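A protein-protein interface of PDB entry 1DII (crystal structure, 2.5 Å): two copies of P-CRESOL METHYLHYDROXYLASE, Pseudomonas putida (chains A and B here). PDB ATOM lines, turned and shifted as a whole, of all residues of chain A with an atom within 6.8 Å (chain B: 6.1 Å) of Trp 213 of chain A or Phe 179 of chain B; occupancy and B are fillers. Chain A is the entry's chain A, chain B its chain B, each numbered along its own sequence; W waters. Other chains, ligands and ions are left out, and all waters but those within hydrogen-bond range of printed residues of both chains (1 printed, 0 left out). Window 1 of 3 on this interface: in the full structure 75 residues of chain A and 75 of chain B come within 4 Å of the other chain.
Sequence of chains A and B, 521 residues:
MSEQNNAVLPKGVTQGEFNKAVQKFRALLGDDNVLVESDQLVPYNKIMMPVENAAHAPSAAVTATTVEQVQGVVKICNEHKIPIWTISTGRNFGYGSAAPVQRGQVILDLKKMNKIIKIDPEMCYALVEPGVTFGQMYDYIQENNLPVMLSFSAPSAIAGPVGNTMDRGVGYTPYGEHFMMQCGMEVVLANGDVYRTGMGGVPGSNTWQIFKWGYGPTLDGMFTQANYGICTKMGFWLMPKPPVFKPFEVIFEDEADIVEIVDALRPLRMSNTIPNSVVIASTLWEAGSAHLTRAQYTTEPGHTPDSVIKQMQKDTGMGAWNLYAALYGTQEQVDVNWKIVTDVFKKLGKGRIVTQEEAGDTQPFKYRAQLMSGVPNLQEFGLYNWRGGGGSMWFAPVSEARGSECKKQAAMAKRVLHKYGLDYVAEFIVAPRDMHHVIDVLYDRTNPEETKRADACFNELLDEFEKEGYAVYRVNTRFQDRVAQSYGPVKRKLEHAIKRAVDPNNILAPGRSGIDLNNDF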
ATOM      1  N   MET A 180       3.813   6.673 -26.981  1.00  0.00           N
ATOM      2  CA  MET A 180       5.028   7.417 -26.680  1.00  0.00           C
ATOM      3  C   MET A 180       5.766   7.766 -27.994  1.00  0.00           C
ATOM      4  O   MET A 180       6.427   8.800 -28.092  1.00  0.00           O
ATOM      5  CB  MET A 180       5.902   6.568 -25.767  1.00  0.00           C
ATOM      6  CG  MET A 180       7.105   7.240 -25.162  1.00  0.00           C
ATOM      7  SD  MET A 180       7.188   6.821 -23.426  1.00  0.00           S
ATOM      8  CE  MET A 180       6.993   8.455 -22.728  1.00  0.00           C
ATOM      9  N   CYS A 183       3.460  10.986 -33.034  1.00  0.00           N
ATOM     10  CA  CYS A 183       3.853  12.372 -33.227  1.00  0.00           C
ATOM     11  C   CYS A 183       2.994  12.964 -34.317  1.00  0.00           C
ATOM     12  O   CYS A 183       3.170  12.671 -35.499  1.00  0.00           O
ATOM     13  CB  CYS A 183       5.335  12.503 -33.609  1.00  0.00           C
ATOM     14  SG  CYS A 183       5.927  14.214 -33.596  1.00  0.00           S
ATOM     15  N   THR A 197      -2.809  18.446 -34.221  1.00  0.00           N
ATOM     16  CA  THR A 197      -2.006  18.594 -33.006  1.00  0.00           C
ATOM     17  C   THR A 197      -0.581  19.022 -33.304  1.00  0.00           C
ATOM     18  O   THR A 197      -0.180  19.043 -34.468  1.00  0.00           O
ATOM     19  CB  THR A 197      -1.920  17.265 -32.260  1.00  0.00           C
ATOM     20  OG1 THR A 197      -1.265  16.255 -33.077  1.00  0.00           O
ATOM     21  CG2 THR A 197      -3.312  16.822 -31.809  1.00  0.00           C
ATOM     22  N   GLY A 198       0.166  19.369 -32.254  1.00  0.00           N
ATOM     23  CA  GLY A 198       1.566  19.740 -32.393  1.00  0.00           C
ATOM     24  C   GLY A 198       1.933  20.811 -33.405  1.00  0.00           C
ATOM     25  O   GLY A 198       1.481  21.944 -33.285  1.00  0.00           O
ATOM     26  N   MET A 199       2.725  20.446 -34.414  1.00  0.00           N
ATOM     27  CA  MET A 199       3.151  21.412 -35.426  1.00  0.00           C
ATOM     28  C   MET A 199       2.270  21.490 -36.696  1.00  0.00           C
ATOM     29  O   MET A 199       2.467  22.358 -37.552  1.00  0.00           O
ATOM     30  CB  MET A 199       4.617  21.167 -35.828  1.00  0.00           C
ATOM     31  CG  MET A 199       5.661  21.238 -34.715  1.00  0.00           C
ATOM     32  SD  MET A 199       5.575  22.648 -33.638  1.00  0.00           S
ATOM     33  CE  MET A 199       6.047  24.020 -34.697  1.00  0.00           C
ATOM     34  N   PHE A 211       8.429  17.144 -34.041  1.00  0.00           N
ATOM     35  CA  PHE A 211       8.305  17.675 -32.674  1.00  0.00           C
ATOM     36  C   PHE A 211       6.875  17.423 -32.171  1.00  0.00           C
ATOM     37  O   PHE A 211       5.911  17.960 -32.721  1.00  0.00           O
ATOM     38  CB  PHE A 211       8.655  19.165 -32.657  1.00  0.00           C
ATOM     39  CG  PHE A 211       8.718  19.761 -31.288  1.00  0.00           C
ATOM     40  CD1 PHE A 211       9.681  19.319 -30.352  1.00  0.00           C
ATOM     41  CD2 PHE A 211       7.795  20.768 -30.906  1.00  0.00           C
ATOM     42  CE1 PHE A 211       9.731  19.874 -29.047  1.00  0.00           C
ATOM     43  CE2 PHE A 211       7.829  21.328 -29.607  1.00  0.00           C
ATOM     44  CZ  PHE A 211       8.802  20.884 -28.671  1.00  0.00           C
ATOM     45  N   LYS A 212       6.774  16.647 -31.089  1.00  0.00           N
ATOM     46  CA  LYS A 212       5.512  16.211 -30.503  1.00  0.00           C
ATOM     47  C   LYS A 212       4.546  17.224 -29.963  1.00  0.00           C
ATOM     48  O   LYS A 212       3.377  17.228 -30.333  1.00  0.00           O
ATOM     49  CB  LYS A 212       5.756  15.213 -29.361  1.00  0.00           C
ATOM     50  CG  LYS A 212       5.941  13.787 -29.739  1.00  0.00           C
ATOM     51  CD  LYS A 212       6.216  12.891 -28.545  1.00  0.00           C
ATOM     52  CE  LYS A 212       4.946  12.495 -27.802  1.00  0.00           C
ATOM     53  NZ  LYS A 212       4.066  11.493 -28.423  1.00  0.00           N
ATOM     54  N   TRP A 213       5.060  18.079 -29.089  1.00  0.00           N
ATOM     55  CA  TRP A 213       4.256  19.026 -28.348  1.00  0.00           C
ATOM     56  C   TRP A 213       3.632  20.228 -28.988  1.00  0.00           C
ATOM     57  O   TRP A 213       2.444  20.510 -28.752  1.00  0.00           O
ATOM     58  CB  TRP A 213       5.005  19.474 -27.096  1.00  0.00           C
ATOM     59  CG  TRP A 213       5.965  18.490 -26.478  1.00  0.00           C
ATOM     60  CD1 TRP A 213       7.279  18.712 -26.234  1.00  0.00           C
ATOM     61  CD2 TRP A 213       5.684  17.166 -25.989  1.00  0.00           C
ATOM     62  NE1 TRP A 213       7.843  17.635 -25.624  1.00  0.00           N
ATOM     63  CE2 TRP A 213       6.895  16.664 -25.453  1.00  0.00           C
ATOM     64  CE3 TRP A 213       4.530  16.351 -25.946  1.00  0.00           C
ATOM     65  CZ2 TRP A 213       6.998  15.390 -24.879  1.00  0.00           C
ATOM     66  CZ3 TRP A 213       4.632  15.071 -25.377  1.00  0.00           C
ATOM     67  CH2 TRP A 213       5.868  14.609 -24.849  1.00  0.00           C
ATOM     68  N   GLY A 214       4.430  20.939 -29.777  1.00  0.00           N
ATOM     69  CA  GLY A 214       3.957  22.155 -30.395  1.00  0.00           C
ATOM     70  C   GLY A 214       4.025  23.250 -29.339  1.00  0.00           C
ATOM     71  O   GLY A 214       4.953  23.301 -28.507  1.00  0.00           O
ATOM     72  N   TYR A 215       2.978  24.063 -29.313  1.00  0.00           N
ATOM     73  CA  TYR A 215       2.880  25.183 -28.403  1.00  0.00           C
ATOM     74  C   TYR A 215       1.487  25.194 -27.809  1.00  0.00           C
ATOM     75  O   TYR A 215       0.520  24.916 -28.499  1.00  0.00           O
ATOM     76  CB  TYR A 215       3.181  26.461 -29.193  1.00  0.00           C
ATOM     77  CG  TYR A 215       2.874  27.771 -28.529  1.00  0.00           C
ATOM     78  CD1 TYR A 215       1.607  28.400 -28.717  1.00  0.00           C
ATOM     79  CD2 TYR A 215       3.819  28.378 -27.674  1.00  0.00           C
ATOM     80  CE1 TYR A 215       1.296  29.595 -28.059  1.00  0.00           C
ATOM     81  CE2 TYR A 215       3.512  29.585 -27.004  1.00  0.00           C
ATOM     82  CZ  TYR A 215       2.242  30.182 -27.211  1.00  0.00           C
ATOM     83  OH  TYR A 215       1.938  31.355 -26.594  1.00  0.00           O
ATOM     84  N   GLY A 216       1.396  25.619 -26.553  1.00  0.00           N
ATOM     85  CA  GLY A 216       0.128  25.656 -25.854  1.00  0.00           C
ATOM     86  C   GLY A 216      -0.217  24.266 -25.355  1.00  0.00           C
ATOM     87  O   GLY A 216       0.672  23.407 -25.324  1.00  0.00           O
ATOM     88  N   PRO A 217      -1.468  24.003 -24.936  1.00  0.00           N
ATOM     89  CA  PRO A 217      -1.770  22.645 -24.462  1.00  0.00           C
ATOM     90  C   PRO A 217      -1.544  21.630 -25.585  1.00  0.00           C
ATOM     91  O   PRO A 217      -1.750  21.968 -26.739  1.00  0.00           O
ATOM     92  CB  PRO A 217      -3.246  22.744 -24.028  1.00  0.00           C
ATOM     93  CG  PRO A 217      -3.782  23.978 -24.749  1.00  0.00           C
ATOM     94  CD  PRO A 217      -2.613  24.914 -24.730  1.00  0.00           C
ATOM     95  N   THR A 218      -0.940  20.483 -25.258  1.00  0.00           N
ATOM     96  CA  THR A 218      -0.664  19.429 -26.242  1.00  0.00           C
ATOM     97  C   THR A 218      -1.759  18.396 -26.009  1.00  0.00           C
ATOM     98  O   THR A 218      -1.852  17.787 -24.947  1.00  0.00           O
ATOM     99  CB  THR A 218       0.806  18.891 -26.145  1.00  0.00           C
ATOM    100  OG1 THR A 218       0.985  17.785 -27.041  1.00  0.00           O
ATOM    101  CG2 THR A 218       1.175  18.476 -24.758  1.00  0.00           C
ATOM    102  N   LEU A 219      -2.625  18.265 -27.009  1.00  0.00           N
ATOM    103  CA  LEU A 219      -3.833  17.450 -26.898  1.00  0.00           C
ATOM    104  C   LEU A 219      -3.964  16.061 -27.498  1.00  0.00           C
ATOM    105  O   LEU A 219      -5.060  15.507 -27.487  1.00  0.00           O
ATOM    106  CB  LEU A 219      -5.045  18.309 -27.319  1.00  0.00           C
ATOM    107  CG  LEU A 219      -5.206  19.711 -26.704  1.00  0.00           C
ATOM    108  CD1 LEU A 219      -6.381  20.438 -27.325  1.00  0.00           C
ATOM    109  CD2 LEU A 219      -5.360  19.598 -25.212  1.00  0.00           C
ATOM    110  N   ASP A 220      -2.873  15.464 -27.966  1.00  0.00           N
ATOM    111  CA  ASP A 220      -2.931  14.122 -28.552  1.00  0.00           C
ATOM    112  C   ASP A 220      -3.532  13.111 -27.605  1.00  0.00           C
ATOM    113  O   ASP A 220      -4.383  12.320 -28.007  1.00  0.00           O
ATOM    114  CB  ASP A 220      -1.539  13.647 -28.958  1.00  0.00           C
ATOM    115  CG  ASP A 220      -0.895  14.587 -29.900  1.00  0.00           C
ATOM    116  OD1 ASP A 220      -0.462  15.663 -29.447  1.00  0.00           O
ATOM    117  OD2 ASP A 220      -0.897  14.304 -31.110  1.00  0.00           O
ATOM    118  N   THR B 165       8.773  22.066 -16.172  1.00  0.00           N
ATOM    119  CA  THR B 165       7.942  21.097 -16.894  1.00  0.00           C
ATOM    120  C   THR B 165       6.589  21.684 -17.316  1.00  0.00           C
ATOM    121  O   THR B 165       6.081  21.313 -18.355  1.00  0.00           O
ATOM    122  CB  THR B 165       7.747  19.786 -16.081  1.00  0.00           C
ATOM    123  OG1 THR B 165       9.030  19.246 -15.762  1.00  0.00           O
ATOM    124  CG2 THR B 165       6.961  18.721 -16.865  1.00  0.00           C
ATOM    125  N   ARG B 168       7.164  22.984 -20.374  1.00  0.00           N
ATOM    126  CA  ARG B 168       7.807  21.940 -21.196  1.00  0.00           C
ATOM    127  C   ARG B 168       9.254  22.280 -21.544  1.00  0.00           C
ATOM    128  O   ARG B 168       9.624  22.355 -22.700  1.00  0.00           O
ATOM    129  CB  ARG B 168       6.996  21.594 -22.445  1.00  0.00           C
ATOM    130  CG  ARG B 168       5.651  20.987 -22.146  1.00  0.00           C
ATOM    131  CD  ARG B 168       4.984  20.413 -23.380  1.00  0.00           C
ATOM    132  NE  ARG B 168       4.714  21.413 -24.419  1.00  0.00           N
ATOM    133  CZ  ARG B 168       3.530  21.976 -24.640  1.00  0.00           C
ATOM    134  NH1 ARG B 168       2.472  21.671 -23.893  1.00  0.00           N
ATOM    135  NH2 ARG B 168       3.377  22.790 -25.666  1.00  0.00           N
ATOM    136  N   GLY B 169      10.036  22.562 -20.508  1.00  0.00           N
ATOM    137  CA  GLY B 169      11.439  22.886 -20.657  1.00  0.00           C
ATOM    138  C   GLY B 169      12.282  21.652 -20.905  1.00  0.00           C
ATOM    139  O   GLY B 169      11.775  20.534 -20.866  1.00  0.00           O
ATOM    140  N   GLY B 176      16.590  14.286 -20.635  1.00  0.00           N
ATOM    141  CA  GLY B 176      16.490  15.693 -20.994  1.00  0.00           C
ATOM    142  C   GLY B 176      15.166  16.242 -21.494  1.00  0.00           C
ATOM    143  O   GLY B 176      14.926  17.442 -21.419  1.00  0.00           O
ATOM    144  N   GLU B 177      14.318  15.383 -22.049  1.00  0.00           N
ATOM    145  CA  GLU B 177      13.006  15.815 -22.515  1.00  0.00           C
ATOM    146  C   GLU B 177      12.143  15.641 -21.283  1.00  0.00           C
ATOM    147  O   GLU B 177      11.565  14.583 -21.062  1.00  0.00           O
ATOM    148  CB  GLU B 177      12.520  14.935 -23.673  1.00  0.00           C
ATOM    149  CG  GLU B 177      12.304  15.716 -24.958  1.00  0.00           C
ATOM    150  CD  GLU B 177      11.254  16.820 -24.824  1.00  0.00           C
ATOM    151  OE1 GLU B 177      10.179  16.565 -24.221  1.00  0.00           O
ATOM    152  OE2 GLU B 177      11.509  17.939 -25.327  1.00  0.00           O
ATOM    153  N   HIS B 178      12.061  16.699 -20.486  1.00  0.00           N
ATOM    154  CA  HIS B 178      11.360  16.658 -19.207  1.00  0.00           C
ATOM    155  C   HIS B 178       9.912  16.245 -19.148  1.00  0.00           C
ATOM    156  O   HIS B 178       9.542  15.516 -18.228  1.00  0.00           O
ATOM    157  CB  HIS B 178      11.571  17.951 -18.434  1.00  0.00           C
ATOM    158  CG  HIS B 178      13.001  18.270 -18.166  1.00  0.00           C
ATOM    159  ND1 HIS B 178      13.398  19.483 -17.662  1.00  0.00           N
ATOM    160  CD2 HIS B 178      14.132  17.542 -18.324  1.00  0.00           C
ATOM    161  CE1 HIS B 178      14.710  19.493 -17.522  1.00  0.00           C
ATOM    162  NE2 HIS B 178      15.180  18.326 -17.918  1.00  0.00           N
ATOM    163  N   PHE B 179       9.104  16.698 -20.113  1.00  0.00           N
ATOM    164  CA  PHE B 179       7.681  16.352 -20.149  1.00  0.00           C
ATOM    165  C   PHE B 179       7.476  14.874 -20.528  1.00  0.00           C
ATOM    166  O   PHE B 179       6.515  14.243 -20.093  1.00  0.00           O
ATOM    167  CB  PHE B 179       6.884  17.300 -21.063  1.00  0.00           C
ATOM    168  CG  PHE B 179       5.394  17.060 -21.032  1.00  0.00           C
ATOM    169  CD1 PHE B 179       4.718  16.709 -22.200  1.00  0.00           C
ATOM    170  CD2 PHE B 179       4.688  17.055 -19.814  1.00  0.00           C
ATOM    171  CE1 PHE B 179       3.347  16.323 -22.180  1.00  0.00           C
ATOM    172  CE2 PHE B 179       3.320  16.672 -19.761  1.00  0.00           C
ATOM    173  CZ  PHE B 179       2.654  16.302 -20.946  1.00  0.00           C
ATOM    174  N   MET B 180       8.426  14.323 -21.279  1.00  0.00           N
ATOM    175  CA  MET B 180       8.395  12.925 -21.685  1.00  0.00           C
ATOM    176  C   MET B 180       8.664  12.018 -20.461  1.00  0.00           C
ATOM    177  O   MET B 180       8.162  10.900 -20.395  1.00  0.00           O
ATOM    178  CB  MET B 180       9.448  12.710 -22.758  1.00  0.00           C
ATOM    179  CG  MET B 180       9.432  11.375 -23.431  1.00  0.00           C
ATOM    180  SD  MET B 180       9.630  11.591 -25.188  1.00  0.00           S
ATOM    181  CE  MET B 180       8.062  10.924 -25.744  1.00  0.00           C
ATOM    182  N   MET B 181       9.395  12.547 -19.475  1.00  0.00           N
ATOM    183  CA  MET B 181       9.717  11.810 -18.269  1.00  0.00           C
ATOM    184  C   MET B 181       8.783  12.109 -17.107  1.00  0.00           C
ATOM    185  O   MET B 181       8.925  11.524 -16.033  1.00  0.00           O
ATOM    186  CB  MET B 181      11.193  12.014 -17.899  1.00  0.00           C
ATOM    187  CG  MET B 181      12.169  11.593 -19.017  1.00  0.00           C
ATOM    188  SD  MET B 181      11.802   9.977 -19.793  1.00  0.00           S
ATOM    189  CE  MET B 181      13.343   9.451 -20.374  1.00  0.00           C
ATOM    190  N   GLN B 182       7.807  12.998 -17.332  1.00  0.00           N
ATOM    191  CA  GLN B 182       6.816  13.355 -16.322  1.00  0.00           C
ATOM    192  C   GLN B 182       5.820  12.181 -16.171  1.00  0.00           C
ATOM    193  O   GLN B 182       5.443  11.539 -17.152  1.00  0.00           O
ATOM    194  CB  GLN B 182       6.117  14.667 -16.724  1.00  0.00           C
ATOM    195  CG  GLN B 182       5.051  15.224 -15.749  1.00  0.00           C
ATOM    196  CD  GLN B 182       3.681  14.666 -16.012  1.00  0.00           C
ATOM    197  OE1 GLN B 182       3.331  14.358 -17.155  1.00  0.00           O
ATOM    198  NE2 GLN B 182       2.910  14.483 -14.952  1.00  0.00           N
ATOM    199  N   CYS B 183       5.428  11.882 -14.933  1.00  0.00           N
ATOM    200  CA  CYS B 183       4.481  10.800 -14.664  1.00  0.00           C
ATOM    201  C   CYS B 183       3.649  11.145 -13.459  1.00  0.00           C
ATOM    202  O   CYS B 183       4.122  11.099 -12.338  1.00  0.00           O
ATOM    203  CB  CYS B 183       5.201   9.467 -14.440  1.00  0.00           C
ATOM    204  SG  CYS B 183       4.139   8.001 -14.546  1.00  0.00           S
ATOM    205  N   MET B 185       0.409  13.975 -12.122  1.00  0.00           N
ATOM    206  CA  MET B 185       0.305  15.338 -11.617  1.00  0.00           C
ATOM    207  C   MET B 185      -1.042  15.562 -10.979  1.00  0.00           C
ATOM    208  O   MET B 185      -2.017  14.870 -11.281  1.00  0.00           O
ATOM    209  CB  MET B 185       0.609  16.429 -12.668  1.00  0.00           C
ATOM    210  CG  MET B 185      -0.444  16.674 -13.741  1.00  0.00           C
ATOM    211  SD  MET B 185      -0.211  18.204 -14.681  1.00  0.00           S
ATOM    212  CE  MET B 185       1.260  17.799 -15.646  1.00  0.00           C
ATOM    213  N   LYS B 212       2.182   6.172 -16.839  1.00  0.00           N
ATOM    214  CA  LYS B 212       1.785   7.489 -17.323  1.00  0.00           C
ATOM    215  C   LYS B 212       0.338   7.782 -17.657  1.00  0.00           C
ATOM    216  O   LYS B 212      -0.277   8.719 -17.113  1.00  0.00           O
ATOM    217  CB  LYS B 212       2.601   7.866 -18.560  1.00  0.00           C
ATOM    218  CG  LYS B 212       3.926   8.506 -18.304  1.00  0.00           C
ATOM    219  CD  LYS B 212       4.660   8.827 -19.600  1.00  0.00           C
ATOM    220  CE  LYS B 212       4.246  10.167 -20.215  1.00  0.00           C
ATOM    221  NZ  LYS B 212       4.696  11.424 -19.557  1.00  0.00           N
ATOM    222  N   ASP B 220      -2.387  15.100 -18.842  1.00  0.00           N
ATOM    223  CA  ASP B 220      -1.204  15.831 -18.364  1.00  0.00           C
ATOM    224  C   ASP B 220      -0.797  16.959 -19.317  1.00  0.00           C
ATOM    225  O   ASP B 220      -0.541  18.097 -18.898  1.00  0.00           O
ATOM    226  CB  ASP B 220      -0.014  14.883 -18.198  1.00  0.00           C
ATOM    227  CG  ASP B 220      -0.298  13.771 -17.241  1.00  0.00           C
ATOM    228  OD1 ASP B 220      -1.019  12.830 -17.630  1.00  0.00           O
ATOM    229  OD2 ASP B 220       0.134  13.863 -16.075  1.00  0.00           O
ATOM    230  N   GLY B 221      -0.832  16.637 -20.608  1.00  0.00           N
ATOM    231  CA  GLY B 221      -0.483  17.580 -21.653  1.00  0.00           C
ATOM    232  C   GLY B 221      -1.386  18.777 -21.794  1.00  0.00           C
ATOM    233  O   GLY B 221      -0.928  19.841 -22.195  1.00  0.00           O
ATOM    234  N   MET B 222      -2.655  18.584 -21.434  1.00  0.00           N
ATOM    235  CA  MET B 222      -3.684  19.606 -21.488  1.00  0.00           C
ATOM    236  C   MET B 222      -3.356  20.730 -20.530  1.00  0.00           C
ATOM    237  O   MET B 222      -3.644  21.873 -20.824  1.00  0.00           O
ATOM    238  CB  MET B 222      -5.036  19.008 -21.124  1.00  0.00           C
ATOM    239  CG  MET B 222      -6.213  19.884 -21.533  1.00  0.00           C
ATOM    240  SD  MET B 222      -7.743  19.264 -20.963  1.00  0.00           S
ATOM    241  CE  MET B 222      -7.722  19.819 -19.332  1.00  0.00           C
ATOM    242  N   THR B 224      -0.054  21.466 -19.365  1.00  0.00           N
ATOM    243  CA  THR B 224       1.239  22.093 -19.666  1.00  0.00           C
ATOM    244  C   THR B 224       1.047  23.161 -20.733  1.00  0.00           C
ATOM    245  O   THR B 224       0.318  22.949 -21.722  1.00  0.00           O
ATOM    246  CB  THR B 224       2.337  21.071 -20.118  1.00  0.00           C
ATOM    247  OG1 THR B 224       2.000  20.480 -21.385  1.00  0.00           O
ATOM    248  CG2 THR B 224       2.492  20.005 -19.092  1.00  0.00           C
HETATM  249  O   HOH W   1       6.445  22.846 -26.393  1.00  0.00           O
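NH2 of Arg 168 of chain B is in hydrogen-bond range of O of Gly 214 of chain A, at 3.3 Å. NH2 of Arg 168 of chain B is in hydrogen-bond range of O of Gly 216 of chain A, at 2.8 Å. N of Thr 218 of chain A is in hydrogen-bond range of O of Gly 221 of chain B (3.1 Å). The indole nitrogen of Trp 213 of chain A is in hydrogen-bond range of the side-chain carboxylate of Glu 177 of chain B, 2.9 Å away.
The backbone carbonyl oxygen (O) of Phe 179 of chain B lies within hydrogen-bond range of the side-chain amino group (NZ) of Lys 212 of chain B (3.4 Å). OG1 of Thr 224 of chain B lies within hydrogen-bond range of O of Gly 221 of chain B (3.1 Å). The guanidinium group of Arg 168 of chain B lies within hydrogen-bond range of the side-chain hydroxyl of Thr 224 of chain B (2.8 Å). The backbone NH (N) of Lys 212 of chain A sits at hydrogen-bond distance from the side-chain sulfur (SG) of Cys 183 of chain A, at 3.6 Å. O of Gln 182 of chain B sits at hydrogen-bond distance from NZ of Lys 212 of chain B (2.5 Å). N of Lys 212 of chain B lies within hydrogen-bond range of SG of Cys 183 of chain B, at 3.5 Å.
Met 180 of chain B touches Met 180 of chain A. Met 180 of chain A touches Lys 212 of chain B. CE of Met 180 of chain B touches CD of Lys 212 of chain A, at 3.9 Å. Trp 213 of chain A touches Arg 168 of chain B (CB to NE, 3.3 Å). Arg 168 of chain B touches Tyr 215 of chain A (NH2 to CA, 3.7 Å). Pro 217 of chain A touches Gly 221 of chain B. CB of Pro 217 of chain A touches O of Met 222 of chain B, at 3.3 Å. Thr 218 of chain A touches Arg 168 of chain B. Thr 218 of chain A touches Met 222 of chain B. Leu 219 of chain A touches Met 222 of chain B.
Of the printed residues of chain B, Trp 213 of chain A touches Arg 168, Glu 177 and Phe 179. Of the printed residues of chain A, Phe 179 of chain B touches Trp 213 (3.6 Å) and Thr 218 (3.9999 Å). Of the printed residues of chain B, Lys 212 of chain A touches Met 180. Printed residues of chain B within 4 Å of Tyr 215 of chain A: Arg 168 (3.7 Å). Of the printed residues of chain B, Gly 216 of chain A touches Arg 168 (2.8 Å) and Thr 224 (3.6 Å). Phe 211 of chain A touches none of the printed residues of chain B. Cys 183 of chain A touches none of the printed residues of chain B. The nearest printed residue of chain B that does not touch Trp 213 of chain A is Met 180 of chain B (4.02 Å). The nearest printed residue of chain A that does not touch Phe 179 of chain B is Met 180 of chain A (6.4 Å).
Hydrophobic or aromatic side chains of chain B that line the printed part of chain A: Phe 179, Met 180 and Met 222.
Met 180 of chain B touches its own counterpart, Met 180 of chain A. Met 180 of chain A touches Lys 212 of chain B, and with the chains exchanged Lys 212 of chain A touches Met 180 of chain B. Positions printed for both chains: 180, 183, 212 and 220. Of the 18 pairs that touch across the chains among the printed residues, 3 have their exchanged pair printed and touching as well.
Water W1 bridges O of Gly 214 of chain A (2.6 Å) and NE of Arg 168 of chain B (3.0 Å).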
